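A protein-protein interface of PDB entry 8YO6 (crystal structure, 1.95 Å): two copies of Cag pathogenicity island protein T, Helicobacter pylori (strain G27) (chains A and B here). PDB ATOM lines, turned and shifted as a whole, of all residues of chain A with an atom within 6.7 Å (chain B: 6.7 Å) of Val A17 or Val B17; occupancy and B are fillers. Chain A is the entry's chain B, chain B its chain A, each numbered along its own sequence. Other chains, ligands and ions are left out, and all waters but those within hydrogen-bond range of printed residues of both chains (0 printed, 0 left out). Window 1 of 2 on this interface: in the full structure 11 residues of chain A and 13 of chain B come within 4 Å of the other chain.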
ATOM      1  N   PHE A  15     -11.589 -28.987  -3.300  1.00  0.00           N
ATOM      2  CA  PHE A  15     -10.205 -28.580  -3.504  1.00  0.00           C
ATOM      3  C   PHE A  15      -9.713 -27.645  -2.403  1.00  0.00           C
ATOM      4  O   PHE A  15     -10.487 -26.936  -1.746  1.00  0.00           O
ATOM      5  CB  PHE A  15     -10.003 -27.894  -4.871  1.00  0.00           C
ATOM      6  CG  PHE A  15     -10.657 -26.535  -4.981  1.00  0.00           C
ATOM      7  CD1 PHE A  15     -10.085 -25.406  -4.388  1.00  0.00           C
ATOM      8  CD2 PHE A  15     -11.845 -26.389  -5.671  1.00  0.00           C
ATOM      9  CE1 PHE A  15     -10.691 -24.171  -4.482  1.00  0.00           C
ATOM     10  CE2 PHE A  15     -12.450 -25.150  -5.777  1.00  0.00           C
ATOM     11  CZ  PHE A  15     -11.875 -24.043  -5.174  1.00  0.00           C
ATOM     12  N   MET A  16      -8.387 -27.622  -2.272  1.00  0.00           N
ATOM     13  CA  MET A  16      -7.656 -26.606  -1.529  1.00  0.00           C
ATOM     14  C   MET A  16      -6.468 -26.202  -2.394  1.00  0.00           C
ATOM     15  O   MET A  16      -5.705 -27.065  -2.835  1.00  0.00           O
ATOM     16  CB  MET A  16      -7.166 -27.130  -0.181  1.00  0.00           C
ATOM     17  CG  MET A  16      -8.257 -27.263   0.864  1.00  0.00           C
ATOM     18  SD  MET A  16      -7.594 -27.945   2.397  1.00  0.00           S
ATOM     19  CE  MET A  16      -6.999 -26.384   3.057  1.00  0.00           C
ATOM     20  N   VAL A  17      -6.340 -24.911  -2.684  1.00  0.00           N
ATOM     21  CA  VAL A  17      -5.260 -24.397  -3.518  1.00  0.00           C
ATOM     22  C   VAL A  17      -4.458 -23.395  -2.701  1.00  0.00           C
ATOM     23  O   VAL A  17      -5.004 -22.378  -2.256  1.00  0.00           O
ATOM     24  CB  VAL A  17      -5.791 -23.735  -4.800  1.00  0.00           C
ATOM     25  CG1 VAL A  17      -4.626 -23.104  -5.574  1.00  0.00           C
ATOM     26  CG2 VAL A  17      -6.538 -24.770  -5.651  1.00  0.00           C
ATOM     27  N   GLN A  18      -3.157 -23.631  -2.582  1.00  0.00           N
ATOM     28  CA  GLN A  18      -2.264 -22.700  -1.907  1.00  0.00           C
ATOM     29  C   GLN A  18      -1.342 -22.070  -2.946  1.00  0.00           C
ATOM     30  O   GLN A  18      -0.661 -22.791  -3.690  1.00  0.00           O
ATOM     31  CB  GLN A  18      -1.463 -23.414  -0.824  1.00  0.00           C
ATOM     32  CG  GLN A  18      -0.393 -22.537  -0.217  1.00  0.00           C
ATOM     33  CD  GLN A  18       0.416 -23.267   0.813  1.00  0.00           C
ATOM     34  OE1 GLN A  18       0.022 -23.336   1.961  1.00  0.00           O
ATOM     35  NE2 GLN A  18       1.547 -23.819   0.410  1.00  0.00           N
ATOM     36  N   VAL A  19      -1.334 -20.735  -3.018  1.00  0.00           N
ATOM     37  CA  VAL A  19      -0.483 -20.019  -3.965  1.00  0.00           C
ATOM     38  C   VAL A  19       0.393 -19.020  -3.221  1.00  0.00           C
ATOM     39  O   VAL A  19      -0.039 -18.395  -2.245  1.00  0.00           O
ATOM     40  CB  VAL A  19      -1.298 -19.297  -5.062  1.00  0.00           C
ATOM     41  CG1 VAL A  19      -1.922 -20.295  -6.013  1.00  0.00           C
ATOM     42  CG2 VAL A  19      -2.343 -18.410  -4.447  1.00  0.00           C
ATOM     43  N   LEU A  36      -5.438 -15.237 -12.380  1.00  0.00           N
ATOM     44  CA  LEU A  36      -5.478 -16.545 -11.736  1.00  0.00           C
ATOM     45  C   LEU A  36      -6.121 -16.448 -10.361  1.00  0.00           C
ATOM     46  O   LEU A  36      -6.974 -17.269 -10.002  1.00  0.00           O
ATOM     47  CB  LEU A  36      -4.066 -17.134 -11.650  1.00  0.00           C
ATOM     48  CG  LEU A  36      -3.761 -18.431 -10.879  1.00  0.00           C
ATOM     49  CD1 LEU A  36      -2.384 -18.901 -11.301  1.00  0.00           C
ATOM     50  CD2 LEU A  36      -3.797 -18.321  -9.364  1.00  0.00           C
ATOM     51  N   LEU A  40      -9.595 -18.306  -8.842  1.00  0.00           N
ATOM     52  CA  LEU A  40      -9.598 -19.012  -7.561  1.00  0.00           C
ATOM     53  C   LEU A  40     -10.699 -18.489  -6.643  1.00  0.00           C
ATOM     54  O   LEU A  40     -11.501 -19.268  -6.113  1.00  0.00           O
ATOM     55  CB  LEU A  40      -8.238 -18.856  -6.887  1.00  0.00           C
ATOM     56  CG  LEU A  40      -7.197 -19.935  -7.107  1.00  0.00           C
ATOM     57  CD1 LEU A  40      -5.945 -19.604  -6.293  1.00  0.00           C
ATOM     58  CD2 LEU A  40      -7.783 -21.289  -6.712  1.00  0.00           C
ATOM     59  N   MET A  87      -1.834 -17.340  -0.172  1.00  0.00           N
ATOM     60  CA  MET A  87      -3.282 -17.393  -0.253  1.00  0.00           C
ATOM     61  C   MET A  87      -3.714 -18.847  -0.331  1.00  0.00           C
ATOM     62  O   MET A  87      -3.149 -19.617  -1.109  1.00  0.00           O
ATOM     63  CB  MET A  87      -3.781 -16.617  -1.461  1.00  0.00           C
ATOM     64  CG  MET A  87      -5.265 -16.524  -1.549  1.00  0.00           C
ATOM     65  SD  MET A  87      -5.772 -15.793  -3.125  1.00  0.00           S
ATOM     66  CE  MET A  87      -7.486 -15.522  -2.791  1.00  0.00           C
ATOM     67  N   ILE A  88      -4.682 -19.232   0.499  1.00  0.00           N
ATOM     68  CA  ILE A  88      -5.252 -20.579   0.464  1.00  0.00           C
ATOM     69  C   ILE A  88      -6.740 -20.445   0.172  1.00  0.00           C
ATOM     70  O   ILE A  88      -7.468 -19.785   0.920  1.00  0.00           O
ATOM     71  CB  ILE A  88      -5.016 -21.344   1.776  1.00  0.00           C
ATOM     72  CG1 ILE A  88      -3.532 -21.374   2.111  1.00  0.00           C
ATOM     73  CG2 ILE A  88      -5.523 -22.778   1.652  1.00  0.00           C
ATOM     74  CD1 ILE A  88      -3.255 -21.826   3.545  1.00  0.00           C
ATOM     75  N   ALA A  89      -7.188 -21.058  -0.914  1.00  0.00           N
ATOM     76  CA  ALA A  89      -8.575 -20.972  -1.334  1.00  0.00           C
ATOM     77  C   ALA A  89      -9.196 -22.359  -1.342  1.00  0.00           C
ATOM     78  O   ALA A  89      -8.562 -23.329  -1.764  1.00  0.00           O
ATOM     79  CB  ALA A  89      -8.682 -20.334  -2.727  1.00  0.00           C
ATOM     80  N   SER A  90     -10.446 -22.455  -0.897  1.00  0.00           N
ATOM     81  CA  SER A  90     -11.088 -23.758  -0.816  1.00  0.00           C
ATOM     82  C   SER A  90     -12.576 -23.621  -1.107  1.00  0.00           C
ATOM     83  O   SER A  90     -13.182 -22.581  -0.825  1.00  0.00           O
ATOM     84  CB  SER A  90     -10.883 -24.401   0.562  1.00  0.00           C
ATOM     85  OG  SER A  90     -11.713 -25.551   0.669  1.00  0.00           O
ATOM     86  N   PHE B  15       2.275 -22.942  -6.914  1.00  0.00           N
ATOM     87  CA  PHE B  15       1.001 -23.409  -6.407  1.00  0.00           C
ATOM     88  C   PHE B  15       1.156 -24.808  -5.836  1.00  0.00           C
ATOM     89  O   PHE B  15       2.074 -25.562  -6.190  1.00  0.00           O
ATOM     90  CB  PHE B  15      -0.091 -23.402  -7.491  1.00  0.00           C
ATOM     91  CG  PHE B  15       0.111 -24.443  -8.568  1.00  0.00           C
ATOM     92  CD1 PHE B  15      -0.257 -25.763  -8.365  1.00  0.00           C
ATOM     93  CD2 PHE B  15       0.679 -24.089  -9.786  1.00  0.00           C
ATOM     94  CE1 PHE B  15      -0.062 -26.725  -9.357  1.00  0.00           C
ATOM     95  CE2 PHE B  15       0.877 -25.041 -10.790  1.00  0.00           C
ATOM     96  CZ  PHE B  15       0.511 -26.362 -10.563  1.00  0.00           C
ATOM     97  N   MET B  16       0.222 -25.142  -4.951  1.00  0.00           N
ATOM     98  CA  MET B  16       0.003 -26.521  -4.539  1.00  0.00           C
ATOM     99  C   MET B  16      -1.505 -26.708  -4.473  1.00  0.00           C
ATOM    100  O   MET B  16      -2.193 -25.929  -3.819  1.00  0.00           O
ATOM    101  CB  MET B  16       0.724 -26.811  -3.212  1.00  0.00           C
ATOM    102  CG  MET B  16       0.316 -28.066  -2.440  1.00  0.00           C
ATOM    103  SD  MET B  16       1.224 -28.172  -0.835  1.00  0.00           S
ATOM    104  CE  MET B  16       2.697 -27.258  -1.203  1.00  0.00           C
ATOM    105  N   VAL B  17      -2.028 -27.688  -5.212  1.00  0.00           N
ATOM    106  CA  VAL B  17      -3.462 -27.941  -5.308  1.00  0.00           C
ATOM    107  C   VAL B  17      -3.719 -29.321  -4.718  1.00  0.00           C
ATOM    108  O   VAL B  17      -3.070 -30.298  -5.108  1.00  0.00           O
ATOM    109  CB  VAL B  17      -3.976 -27.878  -6.766  1.00  0.00           C
ATOM    110  CG1 VAL B  17      -5.454 -28.278  -6.834  1.00  0.00           C
ATOM    111  CG2 VAL B  17      -3.786 -26.491  -7.375  1.00  0.00           C
ATOM    112  N   GLN B  18      -4.617 -29.395  -3.751  1.00  0.00           N
ATOM    113  CA  GLN B  18      -5.026 -30.668  -3.159  1.00  0.00           C
ATOM    114  C   GLN B  18      -6.482 -30.915  -3.519  1.00  0.00           C
ATOM    115  O   GLN B  18      -7.343 -30.096  -3.188  1.00  0.00           O
ATOM    116  CB  GLN B  18      -4.846 -30.644  -1.644  1.00  0.00           C
ATOM    117  CG  GLN B  18      -5.357 -31.921  -0.913  1.00  0.00           C
ATOM    118  CD  GLN B  18      -4.844 -31.983   0.489  1.00  0.00           C
ATOM    119  OE1 GLN B  18      -3.775 -31.441   0.774  1.00  0.00           O
ATOM    120  NE2 GLN B  18      -5.595 -32.633   1.392  1.00  0.00           N
ATOM    121  N   VAL B  19      -6.767 -32.039  -4.178  1.00  0.00           N
ATOM    122  CA  VAL B  19      -8.140 -32.354  -4.540  1.00  0.00           C
ATOM    123  C   VAL B  19      -8.497 -33.731  -4.007  1.00  0.00           C
ATOM    124  O   VAL B  19      -7.639 -34.614  -3.880  1.00  0.00           O
ATOM    125  CB  VAL B  19      -8.391 -32.304  -6.067  1.00  0.00           C
ATOM    126  CG1 VAL B  19      -8.331 -30.859  -6.584  1.00  0.00           C
ATOM    127  CG2 VAL B  19      -7.421 -33.227  -6.807  1.00  0.00           C
ATOM    128  N   LEU B  36     -10.347 -31.877 -15.440  1.00  0.00           N
ATOM    129  CA  LEU B  36      -9.698 -31.041 -14.426  1.00  0.00           C
ATOM    130  C   LEU B  36      -8.379 -31.665 -13.964  1.00  0.00           C
ATOM    131  O   LEU B  36      -7.361 -30.971 -13.870  1.00  0.00           O
ATOM    132  CB  LEU B  36     -10.658 -30.804 -13.245  1.00  0.00           C
ATOM    133  CG  LEU B  36     -10.164 -30.233 -11.893  1.00  0.00           C
ATOM    134  CD1 LEU B  36      -9.458 -28.886 -12.052  1.00  0.00           C
ATOM    135  CD2 LEU B  36     -11.324 -30.085 -10.927  1.00  0.00           C
ATOM    136  N   LEU B  40      -4.533 -30.094 -14.212  1.00  0.00           N
ATOM    137  CA  LEU B  40      -3.564 -30.048 -13.112  1.00  0.00           C
ATOM    138  C   LEU B  40      -2.242 -30.684 -13.513  1.00  0.00           C
ATOM    139  O   LEU B  40      -1.173 -30.109 -13.296  1.00  0.00           O
ATOM    140  CB  LEU B  40      -4.115 -30.750 -11.869  1.00  0.00           C
ATOM    141  CG  LEU B  40      -5.112 -30.000 -11.017  1.00  0.00           C
ATOM    142  CD1 LEU B  40      -5.422 -30.858  -9.761  1.00  0.00           C
ATOM    143  CD2 LEU B  40      -4.540 -28.621 -10.622  1.00  0.00           C
ATOM    144  N   MET B  87      -5.152 -36.206  -4.177  1.00  0.00           N
ATOM    145  CA  MET B  87      -4.087 -35.896  -5.113  1.00  0.00           C
ATOM    146  C   MET B  87      -3.557 -34.497  -4.815  1.00  0.00           C
ATOM    147  O   MET B  87      -4.334 -33.552  -4.649  1.00  0.00           O
ATOM    148  CB  MET B  87      -4.598 -36.055  -6.557  1.00  0.00           C
ATOM    149  CG  MET B  87      -3.734 -35.491  -7.669  1.00  0.00           C
ATOM    150  SD  MET B  87      -4.633 -35.363  -9.248  1.00  0.00           S
ATOM    151  CE  MET B  87      -3.395 -34.537 -10.246  1.00  0.00           C
ATOM    152  N   ILE B  88      -2.243 -34.371  -4.715  1.00  0.00           N
ATOM    153  CA  ILE B  88      -1.596 -33.083  -4.487  1.00  0.00           C
ATOM    154  C   ILE B  88      -0.701 -32.792  -5.680  1.00  0.00           C
ATOM    155  O   ILE B  88       0.190 -33.590  -6.005  1.00  0.00           O
ATOM    156  CB  ILE B  88      -0.793 -33.053  -3.178  1.00  0.00           C
ATOM    157  CG1 ILE B  88      -1.713 -33.388  -1.999  1.00  0.00           C
ATOM    158  CG2 ILE B  88      -0.203 -31.653  -2.977  1.00  0.00           C
ATOM    159  CD1 ILE B  88      -0.981 -33.630  -0.704  1.00  0.00           C
ATOM    160  N   ALA B  89      -0.953 -31.666  -6.349  1.00  0.00           N
ATOM    161  CA  ALA B  89      -0.213 -31.288  -7.538  1.00  0.00           C
ATOM    162  C   ALA B  89       0.480 -29.962  -7.270  1.00  0.00           C
ATOM    163  O   ALA B  89      -0.111 -29.056  -6.681  1.00  0.00           O
ATOM    164  CB  ALA B  89      -1.148 -31.191  -8.765  1.00  0.00           C
ATOM    165  N   SER B  90       1.724 -29.844  -7.715  1.00  0.00           N
ATOM    166  CA  SER B  90       2.512 -28.659  -7.411  1.00  0.00           C
ATOM    167  C   SER B  90       3.469 -28.387  -8.554  1.00  0.00           C
ATOM    168  O   SER B  90       3.902 -29.318  -9.241  1.00  0.00           O
ATOM    169  CB  SER B  90       3.307 -28.854  -6.113  1.00  0.00           C
ATOM    170  OG  SER B  90       4.032 -27.677  -5.836  1.00  0.00           O
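Printed residues of chain B within 4 Å of Val A17: Met B16 and Val B17. Val B17 touches two residues of chain A. Of the printed residues of chain B, Val A19 touches Phe B15 (3.9 Å). Printed residues of chain A within 4 Å of Phe B15: Gln A18 (3.2 Å) and Val A19 (3.9 Å). Of the printed residues of chain B, Phe A15 touches Gln B18 and Val B19. Of the printed residues of chain B, Gln A18 touches Phe B15 and Met B16.
N of Val B19 sits at hydrogen-bond distance from O of Met B87 (2.9 Å). N of Val B17 lies within hydrogen-bond range of O of Ala B89. The backbone carbonyl oxygen of Phe A15 lies within hydrogen-bond range of the side-chain hydroxyl of Ser A90. The backbone carbonyl oxygen (O) of Met A87 sits at hydrogen-bond distance from the backbone NH (N) of Val A19 (2.9 Å). The side-chain hydroxyl (OG) of Ser B90 is in hydrogen-bond range of the backbone carbonyl oxygen (O) of Phe B15. The backbone carbonyl oxygen of Ala A89 is in hydrogen-bond range of the backbone NH of Val A17 (2.9 Å).
Phe A15 touches Val B19, and with the chains exchanged Val A19 touches Phe B15. Met A16 touches its own counterpart, Met B16. Met A16 touches Val B17, and with the chains exchanged Val A17 touches Met B16. Val B17 touches its own counterpart, Val A17. Positions printed for both chains: 15, 16, 17, 18, 19, 36, 40, 87, 88, 89 and 90.
Printed residues of chain B that touch a printed residue of chain A: Phe B15, Met B16, Val B17, Gln B18 and Val B19. Printed residues of chain A that touch a printed residue of chain B: Phe A15, Met A16, Val A17, Gln A18 and Val A19. Hydrophobic or aromatic side chains of chain A that line the printed part of chain B: Phe A15, Val A17 and Val A19. Along chain A the printed residues that touch a printed residue of chain B span positions 15 to 19. Among the printed residues, 10 pairs touch across the chains. Among the printed residues, no Asp or Glu carboxylate lies within 4 Å of a Lys or Arg side-chain nitrogen of the other chain.
Gln B18 touches Phe A15 (O to CA, 3.3 Å). Val B19 touches Phe A15 (CG1 to CB, 3.8 Å). O of Met B16 touches O of Met A16, 3.8 Å away. Met A16 touches Val B17. Val A17 touches Met B16 (CA to O, 3.4 Å). Val B17 touches Val A17 (CG2 to CG2, 3.7 Å). Phe B15 touches Gln A18. Val A19 touches Phe B15.
The backbone carbonyl oxygen (O) of Met B16 is in hydrogen-bond range of the backbone NH (N) of Gln A18, at 2.8 Å. The backbone carbonyl oxygen of Met A16 is in hydrogen-bond range of the backbone NH of Gln B18, 2.7 Å away.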
